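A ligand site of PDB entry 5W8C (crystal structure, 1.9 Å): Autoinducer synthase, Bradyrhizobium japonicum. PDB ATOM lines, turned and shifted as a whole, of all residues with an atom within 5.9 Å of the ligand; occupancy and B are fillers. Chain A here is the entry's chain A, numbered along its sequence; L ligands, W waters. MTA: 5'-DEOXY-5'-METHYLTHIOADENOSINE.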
ATOM      1  N   TRP A  36      26.203 -20.056  -8.492  1.00  0.00           N
ATOM      2  CA  TRP A  36      25.457 -19.148  -7.633  1.00  0.00           C
ATOM      3  C   TRP A  36      24.033 -19.675  -7.507  1.00  0.00           C
ATOM      4  O   TRP A  36      23.093 -19.146  -8.110  1.00  0.00           O
ATOM      5  CB  TRP A  36      25.499 -17.707  -8.143  1.00  0.00           C
ATOM      6  CG  TRP A  36      26.888 -17.076  -8.082  1.00  0.00           C
ATOM      7  CD1 TRP A  36      28.027 -17.642  -7.551  1.00  0.00           C
ATOM      8  CD2 TRP A  36      27.254 -15.765  -8.522  1.00  0.00           C
ATOM      9  NE1 TRP A  36      29.082 -16.764  -7.667  1.00  0.00           N
ATOM     10  CE2 TRP A  36      28.640 -15.606  -8.244  1.00  0.00           C
ATOM     11  CE3 TRP A  36      26.558 -14.711  -9.128  1.00  0.00           C
ATOM     12  CZ2 TRP A  36      29.330 -14.430  -8.567  1.00  0.00           C
ATOM     13  CZ3 TRP A  36      27.242 -13.538  -9.438  1.00  0.00           C
ATOM     14  CH2 TRP A  36      28.619 -13.411  -9.157  1.00  0.00           C
ATOM     15  N   GLU A  37      23.896 -20.729  -6.701  1.00  0.00           N
ATOM     16  CA  GLU A  37      22.667 -21.532  -6.619  1.00  0.00           C
ATOM     17  C   GLU A  37      21.404 -20.781  -6.230  1.00  0.00           C
ATOM     18  O   GLU A  37      20.308 -21.159  -6.647  1.00  0.00           O
ATOM     19  CB  GLU A  37      22.870 -22.731  -5.693  1.00  0.00           C
ATOM     20  CG  GLU A  37      23.793 -23.803  -6.251  1.00  0.00           C
ATOM     21  CD  GLU A  37      23.275 -24.433  -7.541  1.00  0.00           C
ATOM     22  OE1 GLU A  37      22.047 -24.558  -7.723  1.00  0.00           O
ATOM     23  OE2 GLU A  37      24.122 -24.803  -8.379  1.00  0.00           O
ATOM     24  N   THR A  38      21.541 -19.716  -5.446  1.00  0.00           N
ATOM     25  CA  THR A  38      20.378 -18.939  -5.041  1.00  0.00           C
ATOM     26  C   THR A  38      19.670 -18.296  -6.243  1.00  0.00           C
ATOM     27  O   THR A  38      18.519 -17.877  -6.119  1.00  0.00           O
ATOM     28  CB  THR A  38      20.700 -17.891  -3.943  1.00  0.00           C
ATOM     29  OG1 THR A  38      19.491 -17.533  -3.255  1.00  0.00           O
ATOM     30  CG2 THR A  38      21.321 -16.633  -4.538  1.00  0.00           C
ATOM     31  N   LEU A  39      20.352 -18.260  -7.390  1.00  0.00           N
ATOM     32  CA  LEU A  39      19.799 -17.643  -8.599  1.00  0.00           C
ATOM     33  C   LEU A  39      19.151 -18.653  -9.542  1.00  0.00           C
ATOM     34  O   LEU A  39      18.610 -18.258 -10.579  1.00  0.00           O
ATOM     35  CB  LEU A  39      20.893 -16.866  -9.339  1.00  0.00           C
ATOM     36  CG  LEU A  39      21.628 -15.761  -8.563  1.00  0.00           C
ATOM     37  CD1 LEU A  39      22.756 -15.194  -9.410  1.00  0.00           C
ATOM     38  CD2 LEU A  39      20.662 -14.682  -8.115  1.00  0.00           C
ATOM     39  N   ASP A  48      16.432 -11.551 -11.609  1.00  0.00           N
ATOM     40  CA  ASP A  48      16.260 -11.246 -10.181  1.00  0.00           C
ATOM     41  C   ASP A  48      15.419  -9.969  -9.991  1.00  0.00           C
ATOM     42  O   ASP A  48      14.885  -9.427 -10.961  1.00  0.00           O
ATOM     43  CB  ASP A  48      17.620 -11.210  -9.444  1.00  0.00           C
ATOM     44  CG  ASP A  48      18.470  -9.986  -9.808  1.00  0.00           C
ATOM     45  OD1 ASP A  48      17.986  -9.062 -10.489  1.00  0.00           O
ATOM     46  OD2 ASP A  48      19.650  -9.963  -9.383  1.00  0.00           O
ATOM     47  N   SER A  49      15.321  -9.501  -8.747  1.00  0.00           N
ATOM     48  CA  SER A  49      14.502  -8.344  -8.408  1.00  0.00           C
ATOM     49  C   SER A  49      14.987  -7.032  -9.051  1.00  0.00           C
ATOM     50  O   SER A  49      14.259  -6.047  -9.067  1.00  0.00           O
ATOM     51  CB  SER A  49      14.424  -8.160  -6.888  1.00  0.00           C
ATOM     52  OG  SER A  49      13.937  -9.335  -6.272  1.00  0.00           O
ATOM     53  N   TYR A  50      16.208  -7.050  -9.571  1.00  0.00           N
ATOM     54  CA  TYR A  50      16.817  -5.848 -10.163  1.00  0.00           C
ATOM     55  C   TYR A  50      16.779  -5.895 -11.692  1.00  0.00           C
ATOM     56  O   TYR A  50      17.433  -5.103 -12.369  1.00  0.00           O
ATOM     57  CB  TYR A  50      18.232  -5.633  -9.584  1.00  0.00           C
ATOM     58  CG  TYR A  50      18.194  -5.827  -8.088  1.00  0.00           C
ATOM     59  CD1 TYR A  50      17.542  -4.900  -7.264  1.00  0.00           C
ATOM     60  CD2 TYR A  50      18.728  -6.969  -7.500  1.00  0.00           C
ATOM     61  CE1 TYR A  50      17.459  -5.094  -5.897  1.00  0.00           C
ATOM     62  CE2 TYR A  50      18.649  -7.177  -6.127  1.00  0.00           C
ATOM     63  CZ  TYR A  50      18.012  -6.235  -5.333  1.00  0.00           C
ATOM     64  OH  TYR A  50      17.929  -6.438  -3.983  1.00  0.00           O
ATOM     65  N   ARG A  71      25.003  -5.010 -16.480  1.00  0.00           N
ATOM     66  CA  ARG A  71      23.788  -4.219 -16.297  1.00  0.00           C
ATOM     67  C   ARG A  71      23.987  -3.120 -15.258  1.00  0.00           C
ATOM     68  O   ARG A  71      24.869  -3.205 -14.408  1.00  0.00           O
ATOM     69  CB  ARG A  71      22.608  -5.105 -15.919  1.00  0.00           C
ATOM     70  CG  ARG A  71      22.745  -5.749 -14.554  1.00  0.00           C
ATOM     71  CD  ARG A  71      21.495  -6.518 -14.126  1.00  0.00           C
ATOM     72  NE  ARG A  71      21.733  -7.028 -12.770  1.00  0.00           N
ATOM     73  CZ  ARG A  71      20.848  -7.666 -12.026  1.00  0.00           C
ATOM     74  NH1 ARG A  71      19.621  -7.922 -12.478  1.00  0.00           N
ATOM     75  NH2 ARG A  71      21.203  -8.064 -10.813  1.00  0.00           N
ATOM     76  N   MET A  80      20.769  -4.202  -4.836  1.00  0.00           N
ATOM     77  CA  MET A  80      21.381  -5.405  -4.281  1.00  0.00           C
ATOM     78  C   MET A  80      22.201  -5.058  -3.048  1.00  0.00           C
ATOM     79  O   MET A  80      22.167  -5.773  -2.046  1.00  0.00           O
ATOM     80  CB  MET A  80      22.244  -6.131  -5.303  1.00  0.00           C
ATOM     81  CG  MET A  80      22.472  -7.593  -4.973  1.00  0.00           C
ATOM     82  SD  MET A  80      23.712  -8.399  -6.015  1.00  0.00           S
ATOM     83  CE  MET A  80      23.214  -7.825  -7.646  1.00  0.00           C
ATOM     84  N   VAL A  84      20.517  -6.733  -0.015  1.00  0.00           N
ATOM     85  CA  VAL A  84      21.143  -8.043   0.171  1.00  0.00           C
ATOM     86  C   VAL A  84      22.468  -7.940   0.935  1.00  0.00           C
ATOM     87  O   VAL A  84      22.744  -8.737   1.835  1.00  0.00           O
ATOM     88  CB  VAL A  84      21.342  -8.785  -1.177  1.00  0.00           C
ATOM     89  CG1 VAL A  84      21.853 -10.198  -0.940  1.00  0.00           C
ATOM     90  CG2 VAL A  84      20.046  -8.814  -1.965  1.00  0.00           C
ATOM     91  N   PHE A  85      23.284  -6.947   0.598  1.00  0.00           N
ATOM     92  CA  PHE A  85      24.629  -6.846   1.165  1.00  0.00           C
ATOM     93  C   PHE A  85      24.956  -5.528   1.883  1.00  0.00           C
ATOM     94  O   PHE A  85      26.071  -5.022   1.729  1.00  0.00           O
ATOM     95  CB  PHE A  85      25.679  -7.070   0.056  1.00  0.00           C
ATOM     96  CG  PHE A  85      25.537  -8.382  -0.664  1.00  0.00           C
ATOM     97  CD1 PHE A  85      25.930  -9.569  -0.060  1.00  0.00           C
ATOM     98  CD2 PHE A  85      25.038  -8.424  -1.961  1.00  0.00           C
ATOM     99  CE1 PHE A  85      25.816 -10.782  -0.726  1.00  0.00           C
ATOM    100  CE2 PHE A  85      24.929  -9.634  -2.640  1.00  0.00           C
ATOM    101  CZ  PHE A  85      25.314 -10.808  -2.019  1.00  0.00           C
ATOM    102  N   ARG A 105      26.381  -8.349 -12.875  1.00  0.00           N
ATOM    103  CA  ARG A 105      26.176  -9.393 -13.893  1.00  0.00           C
ATOM    104  C   ARG A 105      27.092  -9.247 -15.113  1.00  0.00           C
ATOM    105  O   ARG A 105      26.661  -9.429 -16.254  1.00  0.00           O
ATOM    106  CB  ARG A 105      24.692  -9.488 -14.302  1.00  0.00           C
ATOM    107  CG  ARG A 105      23.752  -9.931 -13.181  1.00  0.00           C
ATOM    108  CD  ARG A 105      24.060 -11.325 -12.635  1.00  0.00           C
ATOM    109  NE  ARG A 105      22.879 -11.866 -11.960  1.00  0.00           N
ATOM    110  CZ  ARG A 105      22.512 -11.569 -10.714  1.00  0.00           C
ATOM    111  NH1 ARG A 105      23.245 -10.752  -9.954  1.00  0.00           N
ATOM    112  NH2 ARG A 105      21.392 -12.098 -10.223  1.00  0.00           N
ATOM    113  N   ILE A 140      28.973  -4.865  -5.857  1.00  0.00           N
ATOM    114  CA  ILE A 140      29.382  -5.920  -4.950  1.00  0.00           C
ATOM    115  C   ILE A 140      30.179  -6.906  -5.779  1.00  0.00           C
ATOM    116  O   ILE A 140      29.634  -7.551  -6.668  1.00  0.00           O
ATOM    117  CB  ILE A 140      28.171  -6.663  -4.350  1.00  0.00           C
ATOM    118  CG1 ILE A 140      27.260  -5.693  -3.595  1.00  0.00           C
ATOM    119  CG2 ILE A 140      28.642  -7.798  -3.456  1.00  0.00           C
ATOM    120  CD1 ILE A 140      26.253  -5.013  -4.490  1.00  0.00           C
ATOM    121  N   MET A 141      31.482  -7.011  -5.512  1.00  0.00           N
ATOM    122  CA  MET A 141      32.322  -7.888  -6.325  1.00  0.00           C
ATOM    123  C   MET A 141      33.312  -8.714  -5.508  1.00  0.00           C
ATOM    124  O   MET A 141      33.750  -8.302  -4.435  1.00  0.00           O
ATOM    125  CB  MET A 141      33.084  -7.076  -7.378  1.00  0.00           C
ATOM    126  CG  MET A 141      34.342  -6.397  -6.861  1.00  0.00           C
ATOM    127  SD  MET A 141      34.021  -4.958  -5.821  1.00  0.00           S
ATOM    128  CE  MET A 141      35.595  -4.118  -5.927  1.00  0.00           C
ATOM    129  N   GLU A 142      33.661  -9.880  -6.047  1.00  0.00           N
ATOM    130  CA  GLU A 142      34.688 -10.714  -5.468  1.00  0.00           C
ATOM    131  C   GLU A 142      36.020  -9.983  -5.568  1.00  0.00           C
ATOM    132  O   GLU A 142      36.240  -9.201  -6.501  1.00  0.00           O
ATOM    133  CB  GLU A 142      34.700 -12.085  -6.127  1.00  0.00           C
ATOM    134  CG  GLU A 142      33.474 -12.879  -5.712  1.00  0.00           C
ATOM    135  CD  GLU A 142      33.219 -14.132  -6.516  1.00  0.00           C
ATOM    136  OE1 GLU A 142      33.652 -14.225  -7.680  1.00  0.00           O
ATOM    137  OE2 GLU A 142      32.540 -15.014  -5.983  1.00  0.00           O
ATOM    138  N   VAL A 165      31.337 -14.291   1.384  1.00  0.00           N
ATOM    139  CA  VAL A 165      29.959 -14.459   0.935  1.00  0.00           C
ATOM    140  C   VAL A 165      29.946 -15.822   0.252  1.00  0.00           C
ATOM    141  O   VAL A 165      30.603 -16.006  -0.776  1.00  0.00           O
ATOM    142  CB  VAL A 165      29.523 -13.341  -0.052  1.00  0.00           C
ATOM    143  CG1 VAL A 165      28.161 -13.658  -0.677  1.00  0.00           C
ATOM    144  CG2 VAL A 165      29.463 -11.991   0.652  1.00  0.00           C
ATOM    145  N   GLU A 166      29.228 -16.781   0.843  1.00  0.00           N
ATOM    146  CA  GLU A 166      29.207 -18.153   0.328  1.00  0.00           C
ATOM    147  C   GLU A 166      30.586 -18.632  -0.121  1.00  0.00           C
ATOM    148  O   GLU A 166      30.798 -18.940  -1.299  1.00  0.00           O
ATOM    149  CB  GLU A 166      28.210 -18.285  -0.847  1.00  0.00           C
ATOM    150  CG  GLU A 166      26.752 -18.103  -0.471  1.00  0.00           C
ATOM    151  CD  GLU A 166      26.185 -19.255   0.347  1.00  0.00           C
ATOM    152  OE1 GLU A 166      25.149 -19.050   1.016  1.00  0.00           O
ATOM    153  OE2 GLU A 166      26.755 -20.370   0.320  1.00  0.00           O
ATOM    154  N   THR A 170      34.514 -11.168  -0.782  1.00  0.00           N
ATOM    155  CA  THR A 170      33.657 -10.262  -1.532  1.00  0.00           C
ATOM    156  C   THR A 170      33.690  -8.890  -0.854  1.00  0.00           C
ATOM    157  O   THR A 170      33.920  -8.807   0.353  1.00  0.00           O
ATOM    158  CB  THR A 170      32.219 -10.828  -1.563  1.00  0.00           C
ATOM    159  OG1 THR A 170      32.251 -12.179  -2.036  1.00  0.00           O
ATOM    160  CG2 THR A 170      31.305 -10.004  -2.460  1.00  0.00           C
HETATM  161  CS  MTA L   1      27.416 -10.432  -6.126  1.00  0.00           C
HETATM  162  S5' MTA L   1      28.551 -11.404  -5.188  1.00  0.00           S
HETATM  163  C5' MTA L   1      28.056 -13.050  -5.622  1.00  0.00           C
HETATM  164  C4' MTA L   1      27.039 -13.601  -4.625  1.00  0.00           C
HETATM  165  O4' MTA L   1      25.871 -12.774  -4.656  1.00  0.00           O
HETATM  166  C2' MTA L   1      25.208 -14.788  -5.619  1.00  0.00           C
HETATM  167  O2' MTA L   1      24.350 -15.926  -5.456  1.00  0.00           O
HETATM  168  C3' MTA L   1      26.573 -15.008  -4.990  1.00  0.00           C
HETATM  169  O3' MTA L   1      26.442 -15.764  -3.779  1.00  0.00           O
HETATM  170  C1' MTA L   1      24.711 -13.582  -4.839  1.00  0.00           C
HETATM  171  N9  MTA L   1      23.674 -12.790  -5.551  1.00  0.00           N
HETATM  172  C8  MTA L   1      23.769 -12.223  -6.765  1.00  0.00           C
HETATM  173  N7  MTA L   1      22.628 -11.572  -7.093  1.00  0.00           N
HETATM  174  C5  MTA L   1      21.785 -11.724  -6.050  1.00  0.00           C
HETATM  175  C6  MTA L   1      20.407 -11.302  -5.718  1.00  0.00           C
HETATM  176  N6  MTA L   1      19.663 -10.557  -6.569  1.00  0.00           N
HETATM  177  N1  MTA L   1      19.901 -11.681  -4.508  1.00  0.00           N
HETATM  178  C2  MTA L   1      20.603 -12.408  -3.630  1.00  0.00           C
HETATM  179  N3  MTA L   1      21.857 -12.841  -3.873  1.00  0.00           N
HETATM  180  C4  MTA L   1      22.479 -12.529  -5.039  1.00  0.00           C
HETATM  181  O   HOH W   1      22.636 -14.138  -1.375  1.00  0.00           O
HETATM  182  O   HOH W   2      17.541 -11.222  -3.099  1.00  0.00           O
HETATM  183  O   HOH W   3      30.927 -10.899  -7.445  1.00  0.00           O
HETATM  184  O   HOH W   4      29.033  -9.344  -8.725  1.00  0.00           O
HETATM  185  O   HOH W   5      16.695 -10.530  -6.236  1.00  0.00           O
HETATM  186  O   HOH W   6      26.878  -7.789  -7.926  1.00  0.00           O
HETATM  187  O   HOH W   7      24.323 -18.647  -3.952  1.00  0.00           O
HETATM  188  O   HOH W   8      27.322 -18.946  -4.244  1.00  0.00           O
HETATM  189  O   HOH W   9      25.101 -15.372  -1.546  1.00  0.00           O
HETATM  190  O   HOH W  10      30.763 -13.873  -3.801  1.00  0.00           O
HETATM  191  O   HOH W  11      29.615 -16.357  -3.319  1.00  0.00           O
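A nitrogen (N6) of the ligand lies within hydrogen-bond range of the side-chain carboxylate (OD2) of Asp 48 (2.9 Å). The guanidinium group (NH1) of Arg 105 lies within hydrogen-bond range of a nitrogen (N7) of the ligand, at 3.0 Å.
OD2 of Asp 48 lies within salt-bridge range of NH2 of Arg 105 (2.9 Å). N of Tyr 50 lies within hydrogen-bond range of OD1 of Asp 48, 2.8 Å away. The side-chain carboxylate (OD1) of Asp 48 lies within salt-bridge range of the guanidinium group (NH1) of Arg 71, 2.8 Å away. N of Phe 85 sits at hydrogen-bond distance from O of Met 80 (3.1 Å).
The side-chain sulfur (SD) of Met 80 lies close to a nitrogen (N7) of the ligand (3.5 Å). Trp 36 touches the ligand (CB to O2', 3.4 Å). CG2 of Thr 38 touches O2' of the ligand, at 3.2 Å. Leu 39 touches the ligand (CD2 to C5, 3.8 Å). CE2 of Tyr 50 touches N6 of the ligand (3.6 Å). CG1 of Val 84 touches C2 of the ligand, at 3.7 Å. Phe 85 touches the ligand. Ile 140 touches the ligand. Of the 18 residues printed, 10 come within 4 Å of the ligand. The nearest printed residue that does not touch the ligand is Glu 166 (4.1 Å).
Water W5 bridges N6 of the ligand (3.0 Å) and OG of Ser 49 (3.0 Å). Water W7 lies within hydrogen-bond range of O2' of the ligand (3.1 Å), N of Thr 38 (3.3 Å) and N of Glu 37 (3.5 Å). Water W6 bridges the backbone carbonyl oxygen (O) of Ile 140 (3.0 Å) and the side-chain sulfur (SD) of Met 80 (3.7 Å). Water W11 lies within hydrogen-bond range of the backbone carbonyl oxygen of Val 165 (2.8 Å), an oxygen (O3') of the ligand (3.3 Å) and the backbone carbonyl oxygen of Glu 166 (3.5 Å). Water W3 bridges N of Glu 142 and S5' of the ligand. Water W10 lies within hydrogen-bond range of OG1 of Thr 170 (2.9 Å), OE2 of Glu 142 (3.0 Å) and S5' of the ligand (3.6 Å).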
